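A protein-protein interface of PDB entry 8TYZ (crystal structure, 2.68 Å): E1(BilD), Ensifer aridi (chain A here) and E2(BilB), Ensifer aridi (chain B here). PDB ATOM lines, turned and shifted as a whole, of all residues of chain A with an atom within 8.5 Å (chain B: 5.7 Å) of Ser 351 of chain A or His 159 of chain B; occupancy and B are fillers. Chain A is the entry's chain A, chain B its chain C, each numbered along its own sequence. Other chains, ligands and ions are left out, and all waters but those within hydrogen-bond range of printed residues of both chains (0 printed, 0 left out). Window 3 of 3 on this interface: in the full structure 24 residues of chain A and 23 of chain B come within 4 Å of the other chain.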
ATOM      1  N   MET A 346      16.235   4.782  18.186  1.00  0.00           N
ATOM      2  CA  MET A 346      15.229   4.728  19.242  1.00  0.00           C
ATOM      3  C   MET A 346      15.265   6.001  20.089  1.00  0.00           C
ATOM      4  O   MET A 346      16.340   6.570  20.317  1.00  0.00           O
ATOM      5  CB  MET A 346      15.455   3.515  20.139  1.00  0.00           C
ATOM      6  CG  MET A 346      14.889   2.245  19.560  1.00  0.00           C
ATOM      7  SD  MET A 346      13.097   2.248  19.340  1.00  0.00           S
ATOM      8  CE  MET A 346      12.511   1.913  20.994  1.00  0.00           C
ATOM      9  N   PRO A 347      14.122   6.490  20.545  1.00  0.00           N
ATOM     10  CA  PRO A 347      14.125   7.674  21.400  1.00  0.00           C
ATOM     11  C   PRO A 347      14.520   7.316  22.822  1.00  0.00           C
ATOM     12  O   PRO A 347      14.273   6.207  23.309  1.00  0.00           O
ATOM     13  CB  PRO A 347      12.676   8.162  21.330  1.00  0.00           C
ATOM     14  CG  PRO A 347      11.925   6.946  21.145  1.00  0.00           C
ATOM     15  CD  PRO A 347      12.754   6.022  20.289  1.00  0.00           C
ATOM     16  N   SER A 348      15.176   8.278  23.463  1.00  0.00           N
ATOM     17  CA  SER A 348      15.699   8.147  24.811  1.00  0.00           C
ATOM     18  C   SER A 348      14.716   8.752  25.802  1.00  0.00           C
ATOM     19  O   SER A 348      13.938   9.652  25.470  1.00  0.00           O
ATOM     20  CB  SER A 348      17.073   8.825  24.943  1.00  0.00           C
ATOM     21  OG  SER A 348      17.112  10.095  24.301  1.00  0.00           O
ATOM     22  N   GLY A 349      14.756   8.253  27.020  1.00  0.00           N
ATOM     23  CA  GLY A 349      13.792   8.648  28.003  1.00  0.00           C
ATOM     24  C   GLY A 349      12.764   7.561  28.198  1.00  0.00           C
ATOM     25  O   GLY A 349      12.956   6.398  27.828  1.00  0.00           O
ATOM     26  N   LYS A 350      11.650   7.958  28.802  1.00  0.00           N
ATOM     27  CA  LYS A 350      10.501   7.089  28.981  1.00  0.00           C
ATOM     28  C   LYS A 350       9.249   7.943  28.838  1.00  0.00           C
ATOM     29  O   LYS A 350       9.308   9.178  28.882  1.00  0.00           O
ATOM     30  CB  LYS A 350      10.533   6.363  30.345  1.00  0.00           C
ATOM     31  CG  LYS A 350      11.607   5.259  30.431  1.00  0.00           C
ATOM     32  CD  LYS A 350      11.643   4.555  31.795  1.00  0.00           C
ATOM     33  CE  LYS A 350      12.789   3.519  31.880  1.00  0.00           C
ATOM     34  NZ  LYS A 350      12.753   2.700  33.147  1.00  0.00           N
ATOM     35  N   SER A 351       8.120   7.278  28.624  1.00  0.00           N
ATOM     36  CA  SER A 351       6.855   7.993  28.640  1.00  0.00           C
ATOM     37  C   SER A 351       6.637   8.620  30.015  1.00  0.00           C
ATOM     38  O   SER A 351       6.811   7.964  31.044  1.00  0.00           O
ATOM     39  CB  SER A 351       5.711   7.043  28.264  1.00  0.00           C
ATOM     40  OG  SER A 351       5.721   5.862  29.043  1.00  0.00           O
ATOM     41  N   LYS A 352       6.289   9.901  30.030  1.00  0.00           N
ATOM     42  CA  LYS A 352       6.085  10.669  31.249  1.00  0.00           C
ATOM     43  C   LYS A 352       4.598  10.808  31.550  1.00  0.00           C
ATOM     44  O   LYS A 352       3.754  10.737  30.655  1.00  0.00           O
ATOM     45  CB  LYS A 352       6.733  12.056  31.132  1.00  0.00           C
ATOM     46  CG  LYS A 352       8.235  11.969  30.903  1.00  0.00           C
ATOM     47  CD  LYS A 352       8.901  13.282  30.606  1.00  0.00           C
ATOM     48  CE  LYS A 352      10.274  13.008  30.041  1.00  0.00           C
ATOM     49  NZ  LYS A 352      10.977  14.239  29.631  1.00  0.00           N
ATOM     50  N   ASP A 353       4.279  11.001  32.829  1.00  0.00           N
ATOM     51  CA  ASP A 353       2.890  11.235  33.213  1.00  0.00           C
ATOM     52  C   ASP A 353       2.399  12.535  32.585  1.00  0.00           C
ATOM     53  O   ASP A 353       3.190  13.415  32.252  1.00  0.00           O
ATOM     54  CB  ASP A 353       2.742  11.290  34.743  1.00  0.00           C
ATOM     55  CG  ASP A 353       3.423  10.107  35.461  1.00  0.00           C
ATOM     56  OD1 ASP A 353       3.505   8.998  34.882  1.00  0.00           O
ATOM     57  OD2 ASP A 353       3.866  10.286  36.618  1.00  0.00           O
ATOM     58  N   GLU A 354       1.080  12.646  32.398  1.00  0.00           N
ATOM     59  CA  GLU A 354       0.513  13.849  31.788  1.00  0.00           C
ATOM     60  C   GLU A 354       1.019  15.110  32.492  1.00  0.00           C
ATOM     61  O   GLU A 354       1.490  16.053  31.841  1.00  0.00           O
ATOM     62  CB  GLU A 354      -1.022  13.777  31.819  1.00  0.00           C
ATOM     63  CG  GLU A 354      -1.733  14.767  30.903  1.00  0.00           C
ATOM     64  CD  GLU A 354      -3.213  14.995  31.257  1.00  0.00           C
ATOM     65  OE1 GLU A 354      -3.642  14.703  32.405  1.00  0.00           O
ATOM     66  OE2 GLU A 354      -3.954  15.494  30.375  1.00  0.00           O
ATOM     67  N   GLN A 356       3.701  15.647  34.196  1.00  0.00           N
ATOM     68  CA  GLN A 356       5.120  15.913  33.974  1.00  0.00           C
ATOM     69  C   GLN A 356       5.388  16.337  32.535  1.00  0.00           C
ATOM     70  O   GLN A 356       6.295  17.134  32.277  1.00  0.00           O
ATOM     71  CB  GLN A 356       5.965  14.681  34.323  1.00  0.00           C
ATOM     72  CG  GLN A 356       5.926  14.258  35.814  1.00  0.00           C
ATOM     73  CD  GLN A 356       6.848  15.100  36.735  1.00  0.00           C
ATOM     74  OE1 GLN A 356       7.651  15.907  36.254  1.00  0.00           O
ATOM     75  NE2 GLN A 356       6.728  14.905  38.063  1.00  0.00           N
ATOM     76  N   LEU A 357       4.618  15.812  31.581  1.00  0.00           N
ATOM     77  CA  LEU A 357       4.827  16.217  30.200  1.00  0.00           C
ATOM     78  C   LEU A 357       4.351  17.644  29.974  1.00  0.00           C
ATOM     79  O   LEU A 357       5.050  18.440  29.335  1.00  0.00           O
ATOM     80  CB  LEU A 357       4.116  15.258  29.257  1.00  0.00           C
ATOM     81  CG  LEU A 357       4.331  15.678  27.797  1.00  0.00           C
ATOM     82  CD1 LEU A 357       5.825  15.727  27.471  1.00  0.00           C
ATOM     83  CD2 LEU A 357       3.629  14.760  26.852  1.00  0.00           C
ATOM     84  N   GLU A 360       6.765  20.111  31.371  1.00  0.00           N
ATOM     85  CA  GLU A 360       7.995  20.254  30.590  1.00  0.00           C
ATOM     86  C   GLU A 360       7.767  21.044  29.316  1.00  0.00           C
ATOM     87  O   GLU A 360       8.624  21.844  28.922  1.00  0.00           O
ATOM     88  CB  GLU A 360       8.586  18.895  30.238  1.00  0.00           C
ATOM     89  CG  GLU A 360       9.397  18.286  31.366  1.00  0.00           C
ATOM     90  CD  GLU A 360       9.796  16.832  31.116  1.00  0.00           C
ATOM     91  OE1 GLU A 360       9.728  16.388  29.933  1.00  0.00           O
ATOM     92  OE2 GLU A 360      10.170  16.145  32.114  1.00  0.00           O
ATOM     93  N   ARG A 490      10.491  -1.952  23.289  1.00  0.00           N
ATOM     94  CA  ARG A 490       9.675  -1.133  22.414  1.00  0.00           C
ATOM     95  C   ARG A 490      10.192  -1.069  20.977  1.00  0.00           C
ATOM     96  O   ARG A 490       9.498  -0.525  20.113  1.00  0.00           O
ATOM     97  CB  ARG A 490       9.564   0.268  23.008  1.00  0.00           C
ATOM     98  CG  ARG A 490       9.044   0.242  24.427  1.00  0.00           C
ATOM     99  CD  ARG A 490       8.893   1.630  25.030  1.00  0.00           C
ATOM    100  NE  ARG A 490       9.972   2.538  24.638  1.00  0.00           N
ATOM    101  CZ  ARG A 490      10.996   2.898  25.404  1.00  0.00           C
ATOM    102  NH1 ARG A 490      11.133   2.438  26.638  1.00  0.00           N
ATOM    103  NH2 ARG A 490      11.903   3.745  24.918  1.00  0.00           N
ATOM    104  N   ALA B 140      -1.710  10.937  22.800  1.00  0.00           N
ATOM    105  CA  ALA B 140      -0.665   9.975  22.473  1.00  0.00           C
ATOM    106  C   ALA B 140      -1.284   8.643  22.079  1.00  0.00           C
ATOM    107  O   ALA B 140      -2.249   8.180  22.696  1.00  0.00           O
ATOM    108  CB  ALA B 140       0.285   9.796  23.664  1.00  0.00           C
ATOM    109  N   GLY B 141      -0.721   8.033  21.042  1.00  0.00           N
ATOM    110  CA  GLY B 141      -1.266   6.830  20.444  1.00  0.00           C
ATOM    111  C   GLY B 141      -1.949   7.060  19.116  1.00  0.00           C
ATOM    112  O   GLY B 141      -2.241   6.087  18.413  1.00  0.00           O
ATOM    113  N   HIS B 146       1.248  12.562  17.196  1.00  0.00           N
ATOM    114  CA  HIS B 146       2.683  12.383  17.021  1.00  0.00           C
ATOM    115  C   HIS B 146       3.238  13.135  15.818  1.00  0.00           C
ATOM    116  O   HIS B 146       4.402  13.552  15.839  1.00  0.00           O
ATOM    117  CB  HIS B 146       3.000  10.903  16.922  1.00  0.00           C
ATOM    118  CG  HIS B 146       2.736  10.173  18.196  1.00  0.00           C
ATOM    119  ND1 HIS B 146       3.576  10.255  19.282  1.00  0.00           N
ATOM    120  CD2 HIS B 146       1.710   9.378  18.578  1.00  0.00           C
ATOM    121  CE1 HIS B 146       3.089   9.526  20.272  1.00  0.00           C
ATOM    122  NE2 HIS B 146       1.958   8.979  19.870  1.00  0.00           N
ATOM    123  N   ASP B 154       7.298  13.875  22.471  1.00  0.00           N
ATOM    124  CA  ASP B 154       6.617  12.680  22.971  1.00  0.00           C
ATOM    125  C   ASP B 154       6.488  11.654  21.848  1.00  0.00           C
ATOM    126  O   ASP B 154       5.382  11.281  21.446  1.00  0.00           O
ATOM    127  CB  ASP B 154       5.254  13.061  23.552  1.00  0.00           C
ATOM    128  CG  ASP B 154       4.609  11.936  24.355  1.00  0.00           C
ATOM    129  OD1 ASP B 154       5.262  10.893  24.587  1.00  0.00           O
ATOM    130  OD2 ASP B 154       3.431  12.103  24.749  1.00  0.00           O
ATOM    131  N   PRO B 155       7.610  11.163  21.326  1.00  0.00           N
ATOM    132  CA  PRO B 155       7.560  10.313  20.136  1.00  0.00           C
ATOM    133  C   PRO B 155       6.938   8.964  20.428  1.00  0.00           C
ATOM    134  O   PRO B 155       7.020   8.440  21.537  1.00  0.00           O
ATOM    135  CB  PRO B 155       9.031  10.167  19.749  1.00  0.00           C
ATOM    136  CG  PRO B 155       9.747  10.320  21.021  1.00  0.00           C
ATOM    137  CD  PRO B 155       8.986  11.325  21.821  1.00  0.00           C
ATOM    138  N   TRP B 156       6.330   8.392  19.389  1.00  0.00           N
ATOM    139  CA  TRP B 156       5.479   7.219  19.559  1.00  0.00           C
ATOM    140  C   TRP B 156       6.254   6.017  20.078  1.00  0.00           C
ATOM    141  O   TRP B 156       5.736   5.251  20.901  1.00  0.00           O
ATOM    142  CB  TRP B 156       4.789   6.907  18.229  1.00  0.00           C
ATOM    143  CG  TRP B 156       4.336   5.502  18.064  1.00  0.00           C
ATOM    144  CD1 TRP B 156       4.858   4.571  17.220  1.00  0.00           C
ATOM    145  CD2 TRP B 156       3.268   4.858  18.759  1.00  0.00           C
ATOM    146  NE1 TRP B 156       4.188   3.384  17.346  1.00  0.00           N
ATOM    147  CE2 TRP B 156       3.199   3.536  18.281  1.00  0.00           C
ATOM    148  CE3 TRP B 156       2.363   5.267  19.745  1.00  0.00           C
ATOM    149  CZ2 TRP B 156       2.263   2.625  18.754  1.00  0.00           C
ATOM    150  CZ3 TRP B 156       1.428   4.356  20.209  1.00  0.00           C
ATOM    151  CH2 TRP B 156       1.389   3.056  19.716  1.00  0.00           C
ATOM    152  N   LEU B 157       7.498   5.851  19.637  1.00  0.00           N
ATOM    153  CA  LEU B 157       8.309   4.725  20.081  1.00  0.00           C
ATOM    154  C   LEU B 157       8.564   4.720  21.595  1.00  0.00           C
ATOM    155  O   LEU B 157       9.089   3.727  22.114  1.00  0.00           O
ATOM    156  CB  LEU B 157       9.632   4.718  19.303  1.00  0.00           C
ATOM    157  CG  LEU B 157       9.507   4.444  17.809  1.00  0.00           C
ATOM    158  CD1 LEU B 157      10.842   4.406  17.129  1.00  0.00           C
ATOM    159  CD2 LEU B 157       8.851   3.132  17.662  1.00  0.00           C
ATOM    160  N   LEU B 158       8.216   5.791  22.319  1.00  0.00           N
ATOM    161  CA  LEU B 158       8.193   5.702  23.776  1.00  0.00           C
ATOM    162  C   LEU B 158       6.959   4.956  24.278  1.00  0.00           C
ATOM    163  O   LEU B 158       6.992   4.385  25.372  1.00  0.00           O
ATOM    164  CB  LEU B 158       8.230   7.089  24.396  1.00  0.00           C
ATOM    165  CG  LEU B 158       9.482   7.916  24.170  1.00  0.00           C
ATOM    166  CD1 LEU B 158       9.270   9.304  24.718  1.00  0.00           C
ATOM    167  CD2 LEU B 158      10.704   7.255  24.785  1.00  0.00           C
ATOM    168  N   HIS B 159       5.861   4.955  23.504  1.00  0.00           N
ATOM    169  CA  HIS B 159       4.585   4.394  23.931  1.00  0.00           C
ATOM    170  C   HIS B 159       4.270   3.062  23.287  1.00  0.00           C
ATOM    171  O   HIS B 159       3.286   2.424  23.679  1.00  0.00           O
ATOM    172  CB  HIS B 159       3.440   5.371  23.626  1.00  0.00           C
ATOM    173  CG  HIS B 159       3.616   6.708  24.260  1.00  0.00           C
ATOM    174  ND1 HIS B 159       3.157   7.001  25.526  1.00  0.00           N
ATOM    175  CD2 HIS B 159       4.234   7.827  23.817  1.00  0.00           C
ATOM    176  CE1 HIS B 159       3.486   8.244  25.836  1.00  0.00           C
ATOM    177  NE2 HIS B 159       4.147   8.766  24.818  1.00  0.00           N
ATOM    178  N   ARG B 160       5.059   2.639  22.305  1.00  0.00           N
ATOM    179  CA  ARG B 160       4.804   1.401  21.586  1.00  0.00           C
ATOM    180  C   ARG B 160       4.822   0.202  22.532  1.00  0.00           C
ATOM    181  O   ARG B 160       5.592   0.159  23.493  1.00  0.00           O
ATOM    182  CB  ARG B 160       5.853   1.232  20.489  1.00  0.00           C
ATOM    183  CG  ARG B 160       5.403   0.445  19.307  1.00  0.00           C
ATOM    184  CD  ARG B 160       6.570   0.100  18.410  1.00  0.00           C
ATOM    185  NE  ARG B 160       6.320  -1.211  17.831  1.00  0.00           N
ATOM    186  CZ  ARG B 160       6.747  -2.351  18.355  1.00  0.00           C
ATOM    187  NH1 ARG B 160       7.598  -2.365  19.371  1.00  0.00           N
ATOM    188  NH2 ARG B 160       6.309  -3.506  17.850  1.00  0.00           N
ATOM    189  N   GLY B 161       3.943  -0.766  22.267  1.00  0.00           N
ATOM    190  CA  GLY B 161       3.858  -1.965  23.077  1.00  0.00           C
ATOM    191  C   GLY B 161       3.071  -1.858  24.374  1.00  0.00           C
ATOM    192  O   GLY B 161       2.925  -2.877  25.067  1.00  0.00           O
ATOM    193  N   SER B 162       2.533  -0.682  24.716  1.00  0.00           N
ATOM    194  CA  SER B 162       2.034  -0.415  26.064  1.00  0.00           C
ATOM    195  C   SER B 162       0.514  -0.356  26.164  1.00  0.00           C
ATOM    196  O   SER B 162      -0.012  -0.124  27.258  1.00  0.00           O
ATOM    197  CB  SER B 162       2.638   0.904  26.610  1.00  0.00           C
ATOM    198  OG  SER B 162       1.863   2.052  26.274  1.00  0.00           O
ATOM    199  N   GLY B 163      -0.211  -0.566  25.075  1.00  0.00           N
ATOM    200  CA  GLY B 163      -1.649  -0.489  25.104  1.00  0.00           C
ATOM    201  C   GLY B 163      -2.201   0.824  24.583  1.00  0.00           C
ATOM    202  O   GLY B 163      -3.333   0.855  24.072  1.00  0.00           O
ATOM    203  N   GLU B 164      -1.437   1.908  24.706  1.00  0.00           N
ATOM    204  CA  GLU B 164      -1.778   3.118  23.973  1.00  0.00           C
ATOM    205  C   GLU B 164      -1.747   2.827  22.472  1.00  0.00           C
ATOM    206  O   GLU B 164      -0.934   2.023  21.990  1.00  0.00           O
ATOM    207  CB  GLU B 164      -0.810   4.241  24.336  1.00  0.00           C
ATOM    208  CG  GLU B 164      -0.471   4.250  25.813  1.00  0.00           C
ATOM    209  CD  GLU B 164       0.175   5.546  26.251  1.00  0.00           C
ATOM    210  OE1 GLU B 164      -0.049   6.552  25.538  1.00  0.00           O
ATOM    211  OE2 GLU B 164       0.900   5.565  27.285  1.00  0.00           O
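The guanidinium group (NH1) of Arg 160 of chain B sits at hydrogen-bond distance from the backbone carbonyl oxygen (O) of Arg 490 of chain A (2.7 Å). O of Leu 157 of chain B lies within hydrogen-bond range of NE of Arg 490 of chain A (2.9 Å).
The backbone carbonyl oxygen (O) of His 159 of chain B is in hydrogen-bond range of the side-chain hydroxyl (OG) of Ser 162 of chain B (3.0 Å). ND1 of His 159 of chain B lies within hydrogen-bond range of OE2 of Glu 164 of chain B (3.2 Å). OD1 of Asp 154 of chain B sits at hydrogen-bond distance from NE2 of His 159 of chain B, 2.4 Å away. The backbone carbonyl oxygen (O) of Asp 154 of chain B lies within hydrogen-bond range of a ring nitrogen (ND1) of His 146 of chain B (3.0 Å).
Among the printed residues, merely in contact across the chains: Arg 490 of chain A with Leu 158 of chain B, Leu 357 of chain A with Asp 154 of chain B, Ser 351 of chain A with His 159 of chain B, Pro 347 of chain A with Leu 157 of chain B, Pro 347 of chain A with Pro 155 of chain B, Met 346 of chain A with Leu 157 of chain B, Pro 347 of chain A with Leu 158 of chain B and Gly 349 of chain A with Leu 158 of chain B.
Printed residues of chain B within 4 Å of Pro 347 of chain A: Pro 155 (3.7 Å), Leu 157 (3.5 Å) and Leu 158 (3.9 Å). Of the printed residues of chain B, Gly 349 of chain A touches Leu 158. Of the printed residues of chain B, Ser 351 of chain A touches His 159. Of chain A, only Ser 351 (3.5 Å) comes within 4 Å of His 159 of chain B. The nearest residue of chain A that does not touch His 159 of chain B is Arg 490 of chain A (4.8 Å). The nearest printed residue of chain A that does not touch Asp 154 of chain B is Ser 351 of chain A (5.2 Å).
Of the 13 printed residues of chain A, 6 touch a printed residue of chain B. Of the 14 printed residues of chain B, 6 touch a printed residue of chain A. Hydrophobic or aromatic side chains of chain B within 4 Å of the printed part of chain A: Pro 155, Leu 157, Leu 158 and His 159. Among the printed residues, no Asp or Glu carboxylate lies within 4 Å of a Lys or Arg side-chain nitrogen of the other chain.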
